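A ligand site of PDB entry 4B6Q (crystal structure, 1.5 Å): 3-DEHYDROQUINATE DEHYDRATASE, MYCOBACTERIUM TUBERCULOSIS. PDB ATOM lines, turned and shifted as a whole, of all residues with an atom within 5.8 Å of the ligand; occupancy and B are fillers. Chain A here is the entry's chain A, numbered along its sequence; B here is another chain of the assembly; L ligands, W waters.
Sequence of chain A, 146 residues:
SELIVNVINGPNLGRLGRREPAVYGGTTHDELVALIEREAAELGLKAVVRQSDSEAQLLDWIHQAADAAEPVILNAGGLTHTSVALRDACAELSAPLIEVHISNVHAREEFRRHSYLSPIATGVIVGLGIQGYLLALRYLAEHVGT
An oxygen (O6) of the ligand is in hydrogen-bond range of the side-chain carboxylate (OD2) of Asp 88 of chain B (2.4 Å).
An oxygen (O2) of the ligand sits at hydrogen-bond distance from the backbone NH of Ser 103, 2.9 Å away.
The side-chain hydroxyl (OG) of Ser 103 lies within hydrogen-bond range of an oxygen (O2) of the ligand (2.7 Å).
A ring nitrogen (NE2) of His 81 lies within hydrogen-bond range of an oxygen (O5) of the ligand (2.7 Å).
O3 of the ligand is in hydrogen-bond range of N of Ile 102 (2.8 Å).
The side-chain amide nitrogen of Asn 75 is in hydrogen-bond range of an oxygen (O3) of the ligand.
O6 of the ligand lies within hydrogen-bond range of NH1 of Arg 112 (3.0 Å).
An oxygen (O4) of the ligand sits at hydrogen-bond distance from a ring nitrogen (ND1) of His 101 (3.3 Å).
An oxygen (O6) of the ligand sits at hydrogen-bond distance from the backbone NH (N) of Gly 78 (3.2 Å).
The side-chain carboxylate (OD1) of Asp 88 of chain B lies within salt-bridge range of the guanidinium group (NH1) of Arg 112 (3.0 Å).
The side-chain hydroxyl (OG) of Ser 103 sits at hydrogen-bond distance from the guanidinium group (NH1) of Arg 108 (2.9 Å).
A ring nitrogen (ND1) of His 81 sits close to the backbone carbonyl oxygen of Arg 112.
The side-chain amide oxygen (OD1) of Asn 75 lies within hydrogen-bond range of a ring nitrogen (ND1) of His 101 (3.2 Å).
The backbone NH (N) of Gly 77 lies close to the side-chain amide oxygen (OD1) of Asn 75 (3.2 Å).
OD1 of Asn 75 lies close to O of Val 100 (3.3 Å).
The backbone carbonyl oxygen (O) of Ala 85 of chain B is in hydrogen-bond range of the side-chain amide nitrogen (ND2) of Asn 12.
The backbone carbonyl oxygen (O) of Gly 77 lies within hydrogen-bond range of the side-chain hydroxyl (OG1) of Thr 80.
Asn 12 touches the ligand (O to C1, 3.3 Å).
CD1 of Leu 13 touches C16 of the ligand, at 3.8 Å.
Arg 15 touches the ligand (O to C8, 3.6 Å).
Leu 16 touches the ligand.
Gly 77 touches the ligand.
CG1 of Val 105 touches C13 of the ligand, at 3.8 Å.
CG1 of Val 84 of chain B touches O6 of the ligand, at 3.9 Å.
Hydrophobic or aromatic side chains that line the ligand: Leu 13, Leu 16, His 81, His 101, Ile 102, Val 105 and Val 84 of chain B.
15 residues have an atom within 4 Å of the ligand: Asn 12, Leu 13, Arg 15, Leu 16, Asn 75, Gly 77, Gly 78, His 81, His 101, Ile 102, Ser 103, Val 105, Arg 112, Val 84 of chain B and Asp 88 of chain B.
The nearest printed residue that does not touch the ligand is Pro 11 (4.01 Å).
Water W3 lies within hydrogen-bond range of N of Gly 17 (3.0 Å) and S1 of the ligand (3.3 Å).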
ATOM      1  N   PRO A  11      -1.013  -3.159   9.839  1.00  0.00           N
ATOM      2  CA  PRO A  11      -1.175  -1.835  10.414  1.00  0.00           C
ATOM      3  C   PRO A  11      -2.581  -1.264  10.345  1.00  0.00           C
ATOM      4  O   PRO A  11      -3.332  -1.470   9.379  1.00  0.00           O
ATOM      5  CB  PRO A  11      -0.225  -0.981   9.617  1.00  0.00           C
ATOM      6  CG  PRO A  11       0.739  -1.882   9.037  1.00  0.00           C
ATOM      7  CD  PRO A  11       0.168  -3.251   8.962  1.00  0.00           C
ATOM      8  N   ASN A  12      -2.893  -0.562  11.409  1.00  0.00           N
ATOM      9  CA  ASN A  12      -4.160   0.106  11.602  1.00  0.00           C
ATOM     10  C   ASN A  12      -5.355  -0.786  11.943  1.00  0.00           C
ATOM     11  O   ASN A  12      -6.395  -0.272  12.388  1.00  0.00           O
ATOM     12  CB  ASN A  12      -4.505   1.002  10.408  1.00  0.00           C
ATOM     13  CG  ASN A  12      -3.451   2.081  10.197  1.00  0.00           C
ATOM     14  OD1 ASN A  12      -3.169   2.859  11.116  1.00  0.00           O
ATOM     15  ND2 ASN A  12      -2.920   2.166   9.011  1.00  0.00           N
ATOM     16  N   LEU A  13      -5.208  -2.118  11.839  1.00  0.00           N
ATOM     17  CA  LEU A  13      -6.325  -3.008  12.133  1.00  0.00           C
ATOM     18  C   LEU A  13      -6.664  -2.984  13.637  1.00  0.00           C
ATOM     19  O   LEU A  13      -7.760  -3.350  14.006  1.00  0.00           O
ATOM     20  CB  LEU A  13      -6.047  -4.418  11.637  1.00  0.00           C
ATOM     21  CG  LEU A  13      -6.500  -4.829  10.214  1.00  0.00           C
ATOM     22  CD1 LEU A  13      -8.022  -4.614   9.910  1.00  0.00           C
ATOM     23  CD2 LEU A  13      -5.573  -4.406   9.154  1.00  0.00           C
ATOM     24  N   ARG A  15      -7.309  -0.411  15.128  1.00  0.00           N
ATOM     25  CA  ARG A  15      -8.181   0.783  15.222  1.00  0.00           C
ATOM     26  C   ARG A  15      -9.635   0.434  14.864  1.00  0.00           C
ATOM     27  O   ARG A  15     -10.515   1.316  14.857  1.00  0.00           O
ATOM     28  CB  ARG A  15      -7.667   1.904  14.269  1.00  0.00           C
ATOM     29  CG  ARG A  15      -6.211   2.321  14.434  1.00  0.00           C
ATOM     30  CD  ARG A  15      -6.020   3.005  15.742  1.00  0.00           C
ATOM     31  NE  ARG A  15      -6.777   4.250  15.753  1.00  0.00           N
ATOM     32  CZ  ARG A  15      -7.035   4.958  16.836  1.00  0.00           C
ATOM     33  NH1 ARG A  15      -6.576   4.577  18.010  1.00  0.00           N
ATOM     34  NH2 ARG A  15      -7.756   6.050  16.728  1.00  0.00           N
ATOM     35  N   LEU A  16      -9.925  -0.835  14.551  1.00  0.00           N
ATOM     36  CA  LEU A  16     -11.291  -1.205  14.182  1.00  0.00           C
ATOM     37  C   LEU A  16     -12.274  -0.758  15.263  1.00  0.00           C
ATOM     38  O   LEU A  16     -12.013  -0.925  16.447  1.00  0.00           O
ATOM     39  CB  LEU A  16     -11.362  -2.702  14.025  1.00  0.00           C
ATOM     40  CG  LEU A  16     -10.871  -3.324  12.749  1.00  0.00           C
ATOM     41  CD1 LEU A  16     -10.823  -4.830  12.930  1.00  0.00           C
ATOM     42  CD2 LEU A  16     -11.830  -2.949  11.590  1.00  0.00           C
ATOM     43  N   GLY A  17     -13.378  -0.127  14.854  1.00  0.00           N
ATOM     44  CA  GLY A  17     -14.424   0.286  15.816  1.00  0.00           C
ATOM     45  C   GLY A  17     -14.125   1.475  16.696  1.00  0.00           C
ATOM     46  O   GLY A  17     -14.878   1.741  17.663  1.00  0.00           O
ATOM     47  N   ASN A  75      -4.499 -10.161   6.666  1.00  0.00           N
ATOM     48  CA  ASN A  75      -4.961  -8.856   6.267  1.00  0.00           C
ATOM     49  C   ASN A  75      -3.856  -7.880   6.602  1.00  0.00           C
ATOM     50  O   ASN A  75      -3.756  -7.443   7.737  1.00  0.00           O
ATOM     51  CB  ASN A  75      -6.235  -8.465   6.983  1.00  0.00           C
ATOM     52  CG  ASN A  75      -6.777  -7.119   6.506  1.00  0.00           C
ATOM     53  OD1 ASN A  75      -6.118  -6.421   5.735  1.00  0.00           O
ATOM     54  ND2 ASN A  75      -8.015  -6.796   6.908  1.00  0.00           N
ATOM     55  N   ALA A  76      -3.014  -7.604   5.620  1.00  0.00           N
ATOM     56  CA  ALA A  76      -1.802  -6.843   5.853  1.00  0.00           C
ATOM     57  C   ALA A  76      -2.015  -5.347   5.899  1.00  0.00           C
ATOM     58  O   ALA A  76      -1.042  -4.586   6.059  1.00  0.00           O
ATOM     59  CB  ALA A  76      -0.739  -7.187   4.808  1.00  0.00           C
ATOM     60  N   GLY A  77      -3.273  -4.892   5.824  1.00  0.00           N
ATOM     61  CA  GLY A  77      -3.529  -3.457   5.791  1.00  0.00           C
ATOM     62  C   GLY A  77      -2.790  -2.780   4.674  1.00  0.00           C
ATOM     63  O   GLY A  77      -2.657  -3.325   3.564  1.00  0.00           O
ATOM     64  N   GLY A  78      -2.289  -1.588   4.926  1.00  0.00           N
ATOM     65  CA  GLY A  78      -1.619  -0.856   3.871  1.00  0.00           C
ATOM     66  C   GLY A  78      -0.403  -1.524   3.275  1.00  0.00           C
ATOM     67  O   GLY A  78      -0.024  -1.262   2.119  1.00  0.00           O
ATOM     68  N   LEU A  79       0.215  -2.425   4.040  1.00  0.00           N
ATOM     69  CA  LEU A  79       1.382  -3.165   3.545  1.00  0.00           C
ATOM     70  C   LEU A  79       1.060  -4.091   2.381  1.00  0.00           C
ATOM     71  O   LEU A  79       1.945  -4.467   1.629  1.00  0.00           O
ATOM     72  CB  LEU A  79       2.057  -3.957   4.677  1.00  0.00           C
ATOM     73  CG  LEU A  79       2.546  -3.134   5.864  1.00  0.00           C
ATOM     74  CD1 LEU A  79       3.060  -4.027   6.991  1.00  0.00           C
ATOM     75  CD2 LEU A  79       3.575  -2.064   5.411  1.00  0.00           C
ATOM     76  N   THR A  80      -0.213  -4.448   2.233  1.00  0.00           N
ATOM     77  CA  THR A  80      -0.698  -5.213   1.074  1.00  0.00           C
ATOM     78  C   THR A  80      -0.210  -4.600  -0.220  1.00  0.00           C
ATOM     79  O   THR A  80       0.166  -5.292  -1.171  1.00  0.00           O
ATOM     80  CB  THR A  80      -2.236  -5.200   1.081  1.00  0.00           C
ATOM     81  OG1 THR A  80      -2.679  -5.660   2.349  1.00  0.00           O
ATOM     82  CG2 THR A  80      -2.846  -6.054  -0.042  1.00  0.00           C
ATOM     83  N   HIS A  81      -0.258  -3.266  -0.276  1.00  0.00           N
ATOM     84  CA  HIS A  81      -0.043  -2.545  -1.495  1.00  0.00           C
ATOM     85  C   HIS A  81       1.398  -2.129  -1.705  1.00  0.00           C
ATOM     86  O   HIS A  81       1.740  -1.612  -2.772  1.00  0.00           O
ATOM     87  CB  HIS A  81      -0.948  -1.313  -1.507  1.00  0.00           C
ATOM     88  CG  HIS A  81      -2.350  -1.621  -1.094  1.00  0.00           C
ATOM     89  ND1 HIS A  81      -3.163  -2.458  -1.832  1.00  0.00           N
ATOM     90  CD2 HIS A  81      -3.059  -1.270   0.010  1.00  0.00           C
ATOM     91  CE1 HIS A  81      -4.335  -2.572  -1.216  1.00  0.00           C
ATOM     92  NE2 HIS A  81      -4.285  -1.874  -0.096  1.00  0.00           N
ATOM     93  N   VAL A 100      -7.298 -11.537   3.153  1.00  0.00           N
ATOM     94  CA  VAL A 100      -8.623 -10.985   3.477  1.00  0.00           C
ATOM     95  C   VAL A 100      -8.508  -9.459   3.617  1.00  0.00           C
ATOM     96  O   VAL A 100      -7.591  -8.976   4.275  1.00  0.00           O
ATOM     97  CB  VAL A 100      -9.173 -11.596   4.785  1.00  0.00           C
ATOM     98  CG1 VAL A 100     -10.439 -10.853   5.297  1.00  0.00           C
ATOM     99  CG2 VAL A 100      -9.414 -13.083   4.627  1.00  0.00           C
ATOM    100  N   HIS A 101      -9.433  -8.741   3.002  1.00  0.00           N
ATOM    101  CA  HIS A 101      -9.646  -7.332   3.273  1.00  0.00           C
ATOM    102  C   HIS A 101     -11.102  -7.106   3.642  1.00  0.00           C
ATOM    103  O   HIS A 101     -11.998  -7.695   3.044  1.00  0.00           O
ATOM    104  CB  HIS A 101      -9.227  -6.468   2.087  1.00  0.00           C
ATOM    105  CG  HIS A 101      -7.784  -6.668   1.751  1.00  0.00           C
ATOM    106  ND1 HIS A 101      -6.785  -6.362   2.648  1.00  0.00           N
ATOM    107  CD2 HIS A 101      -7.188  -7.292   0.708  1.00  0.00           C
ATOM    108  CE1 HIS A 101      -5.617  -6.722   2.117  1.00  0.00           C
ATOM    109  NE2 HIS A 101      -5.840  -7.298   0.956  1.00  0.00           N
ATOM    110  N   ILE A 102     -11.318  -6.294   4.649  1.00  0.00           N
ATOM    111  CA  ILE A 102     -12.637  -5.990   5.144  1.00  0.00           C
ATOM    112  C   ILE A 102     -13.410  -5.163   4.095  1.00  0.00           C
ATOM    113  O   ILE A 102     -14.547  -5.484   3.736  1.00  0.00           O
ATOM    114  CB  ILE A 102     -12.488  -5.245   6.508  1.00  0.00           C
ATOM    115  CG1 ILE A 102     -11.891  -6.205   7.556  1.00  0.00           C
ATOM    116  CG2 ILE A 102     -13.816  -4.674   6.980  1.00  0.00           C
ATOM    117  CD1 ILE A 102     -11.530  -5.482   8.832  1.00  0.00           C
ATOM    118  N   SER A 103     -12.771  -4.087   3.628  1.00  0.00           N
ATOM    119  CA  SER A 103     -13.335  -3.227   2.592  1.00  0.00           C
ATOM    120  C   SER A 103     -13.129  -3.804   1.201  1.00  0.00           C
ATOM    121  O   SER A 103     -12.271  -4.658   0.972  1.00  0.00           O
ATOM    122  CB  SER A 103     -12.722  -1.830   2.680  1.00  0.00           C
ATOM    123  OG  SER A 103     -11.393  -1.765   2.230  1.00  0.00           O
ATOM    124  N   ASN A 104     -13.959  -3.362   0.265  1.00  0.00           N
ATOM    125  CA  ASN A 104     -13.763  -3.734  -1.130  1.00  0.00           C
ATOM    126  C   ASN A 104     -12.698  -2.816  -1.701  1.00  0.00           C
ATOM    127  O   ASN A 104     -12.986  -1.697  -2.137  1.00  0.00           O
ATOM    128  CB  ASN A 104     -15.057  -3.654  -1.928  1.00  0.00           C
ATOM    129  CG  ASN A 104     -14.865  -4.130  -3.346  1.00  0.00           C
ATOM    130  OD1 ASN A 104     -13.738  -4.296  -3.785  1.00  0.00           O
ATOM    131  ND2 ASN A 104     -15.961  -4.307  -4.085  1.00  0.00           N
ATOM    132  N   VAL A 105     -11.458  -3.296  -1.699  1.00  0.00           N
ATOM    133  CA  VAL A 105     -10.334  -2.502  -2.180  1.00  0.00           C
ATOM    134  C   VAL A 105     -10.460  -2.115  -3.656  1.00  0.00           C
ATOM    135  O   VAL A 105      -9.760  -1.221  -4.102  1.00  0.00           O
ATOM    136  CB  VAL A 105      -9.027  -3.237  -1.931  1.00  0.00           C
ATOM    137  CG1 VAL A 105      -8.755  -3.312  -0.402  1.00  0.00           C
ATOM    138  CG2 VAL A 105      -9.013  -4.612  -2.631  1.00  0.00           C
ATOM    139  N   ARG A 108     -12.201   1.543  -4.346  1.00  0.00           N
ATOM    140  CA  ARG A 108     -11.534   2.655  -3.689  1.00  0.00           C
ATOM    141  C   ARG A 108     -10.483   3.276  -4.598  1.00  0.00           C
ATOM    142  O   ARG A 108     -10.608   3.218  -5.823  1.00  0.00           O
ATOM    143  CB  ARG A 108     -10.966   2.176  -2.340  1.00  0.00           C
ATOM    144  CG  ARG A 108     -12.059   1.590  -1.433  1.00  0.00           C
ATOM    145  CD  ARG A 108     -11.552   1.143  -0.071  1.00  0.00           C
ATOM    146  NE  ARG A 108     -10.983   2.251   0.679  1.00  0.00           N
ATOM    147  CZ  ARG A 108     -10.351   2.106   1.839  1.00  0.00           C
ATOM    148  NH1 ARG A 108     -10.209   0.901   2.394  1.00  0.00           N
ATOM    149  NH2 ARG A 108      -9.870   3.172   2.439  1.00  0.00           N
ATOM    150  N   ARG A 112      -5.073   0.951  -4.299  1.00  0.00           N
ATOM    151  CA  ARG A 112      -5.543  -0.172  -3.459  1.00  0.00           C
ATOM    152  C   ARG A 112      -5.913  -1.390  -4.279  1.00  0.00           C
ATOM    153  O   ARG A 112      -6.115  -2.466  -3.708  1.00  0.00           O
ATOM    154  CB  ARG A 112      -6.735   0.179  -2.582  1.00  0.00           C
ATOM    155  CG  ARG A 112      -6.426   1.262  -1.585  1.00  0.00           C
ATOM    156  CD  ARG A 112      -7.559   1.432  -0.591  1.00  0.00           C
ATOM    157  NE  ARG A 112      -7.390   2.710   0.069  1.00  0.00           N
ATOM    158  CZ  ARG A 112      -6.586   2.941   1.105  1.00  0.00           C
ATOM    159  NH1 ARG A 112      -5.939   1.954   1.729  1.00  0.00           N
ATOM    160  NH2 ARG A 112      -6.486   4.178   1.570  1.00  0.00           N
ATOM    161  N   TYR A 133     -13.093 -13.070   7.326  1.00  0.00           N
ATOM    162  CA  TYR A 133     -12.184 -13.918   8.095  1.00  0.00           C
ATOM    163  C   TYR A 133     -12.812 -15.248   8.418  1.00  0.00           C
ATOM    164  O   TYR A 133     -12.146 -16.284   8.405  1.00  0.00           O
ATOM    165  CB  TYR A 133     -11.834 -13.269   9.403  1.00  0.00           C
ATOM    166  CG  TYR A 133     -10.994 -12.009   9.320  1.00  0.00           C
ATOM    167  CD1 TYR A 133      -9.617 -12.078   9.334  1.00  0.00           C
ATOM    168  CD2 TYR A 133     -11.575 -10.768   9.297  1.00  0.00           C
ATOM    169  CE1 TYR A 133      -8.850 -10.923   9.315  1.00  0.00           C
ATOM    170  CE2 TYR A 133     -10.825  -9.624   9.220  1.00  0.00           C
ATOM    171  CZ  TYR A 133      -9.463  -9.697   9.266  1.00  0.00           C
ATOM    172  OH  TYR A 133      -8.741  -8.538   9.247  1.00  0.00           O
ATOM    173  N   VAL B  84       1.308   3.571   2.425  1.00  0.00           N
ATOM    174  CA  VAL B  84      -0.147   3.589   2.492  1.00  0.00           C
ATOM    175  C   VAL B  84      -0.590   3.476   3.954  1.00  0.00           C
ATOM    176  O   VAL B  84      -1.570   4.106   4.351  1.00  0.00           O
ATOM    177  CB  VAL B  84      -0.766   2.482   1.603  1.00  0.00           C
ATOM    178  CG1 VAL B  84      -2.275   2.354   1.873  1.00  0.00           C
ATOM    179  CG2 VAL B  84      -0.459   2.733   0.113  1.00  0.00           C
ATOM    180  N   ALA B  85       0.116   2.674   4.758  1.00  0.00           N
ATOM    181  CA  ALA B  85      -0.257   2.526   6.180  1.00  0.00           C
ATOM    182  C   ALA B  85      -0.290   3.885   6.882  1.00  0.00           C
ATOM    183  O   ALA B  85      -1.191   4.142   7.682  1.00  0.00           O
ATOM    184  CB  ALA B  85       0.698   1.562   6.906  1.00  0.00           C
ATOM    185  N   ASP B  88      -3.314   5.832   5.786  1.00  0.00           N
ATOM    186  CA  ASP B  88      -4.524   5.316   6.419  1.00  0.00           C
ATOM    187  C   ASP B  88      -4.674   5.772   7.883  1.00  0.00           C
ATOM    188  O   ASP B  88      -5.779   6.096   8.334  1.00  0.00           O
ATOM    189  CB  ASP B  88      -4.466   3.741   6.556  1.00  0.00           C
ATOM    190  CG  ASP B  88      -4.572   2.944   5.227  1.00  0.00           C
ATOM    191  OD1 ASP B  88      -5.226   3.377   4.249  1.00  0.00           O
ATOM    192  OD2 ASP B  88      -4.030   1.801   5.199  1.00  0.00           O
HETATM  193  C1  LIG L   1      -9.241   0.488  10.834  1.00  0.00           C
HETATM  194  C2  LIG L   1      -9.390  -0.166   9.690  1.00  0.00           C
HETATM  195  C3  LIG L   1      -8.445  -0.902   8.963  1.00  0.00           C
HETATM  196  C4  LIG L   1      -8.809  -1.509   7.798  1.00  0.00           C
HETATM  197  C5  LIG L   1     -10.151  -1.438   7.375  1.00  0.00           C
HETATM  198  C6  LIG L   1     -11.116  -0.739   8.081  1.00  0.00           C
HETATM  199  C7  LIG L   1     -10.744  -0.095   9.239  1.00  0.00           C
HETATM  200  S1  LIG L   1     -11.678   0.820  10.349  1.00  0.00           S
HETATM  201  C8  LIG L   1     -10.305   1.102  11.307  1.00  0.00           C
HETATM  202  O1  LIG L   1      -5.612  -0.823   6.146  1.00  0.00           O
HETATM  203  C9  LIG L   1      -6.420  -1.048   5.244  1.00  0.00           C
HETATM  204  C10 LIG L   1      -7.774  -2.923   4.470  1.00  0.00           C
HETATM  205  C11 LIG L   1      -9.087  -3.686   4.609  1.00  0.00           C
HETATM  206  C12 LIG L   1      -7.706  -1.811   5.521  1.00  0.00           C
HETATM  207  O2  LIG L   1     -10.111  -3.126   4.182  1.00  0.00           O
HETATM  208  O3  LIG L   1      -9.045  -4.796   5.174  1.00  0.00           O
HETATM  209  O4  LIG L   1      -6.672  -3.817   4.702  1.00  0.00           O
HETATM  210  C13 LIG L   1      -7.687  -2.309   3.069  1.00  0.00           C
HETATM  211  C14 LIG L   1      -6.348  -1.609   2.824  1.00  0.00           C
HETATM  212  O5  LIG L   1      -6.314  -1.009   1.480  1.00  0.00           O
HETATM  213  C15 LIG L   1      -6.169  -0.511   3.841  1.00  0.00           C
HETATM  214  O6  LIG L   1      -4.819   0.050   3.730  1.00  0.00           O
HETATM  215  C16 LIG L   1      -7.789  -2.306   6.960  1.00  0.00           C
HETATM  216  O   HOH W   1      -3.153   0.064   7.062  1.00  0.00           O
HETATM  217  O   HOH W   2      -9.560   1.227   5.289  1.00  0.00           O
HETATM  218  O   HOH W   3     -14.447   0.226  12.058  1.00  0.00           O
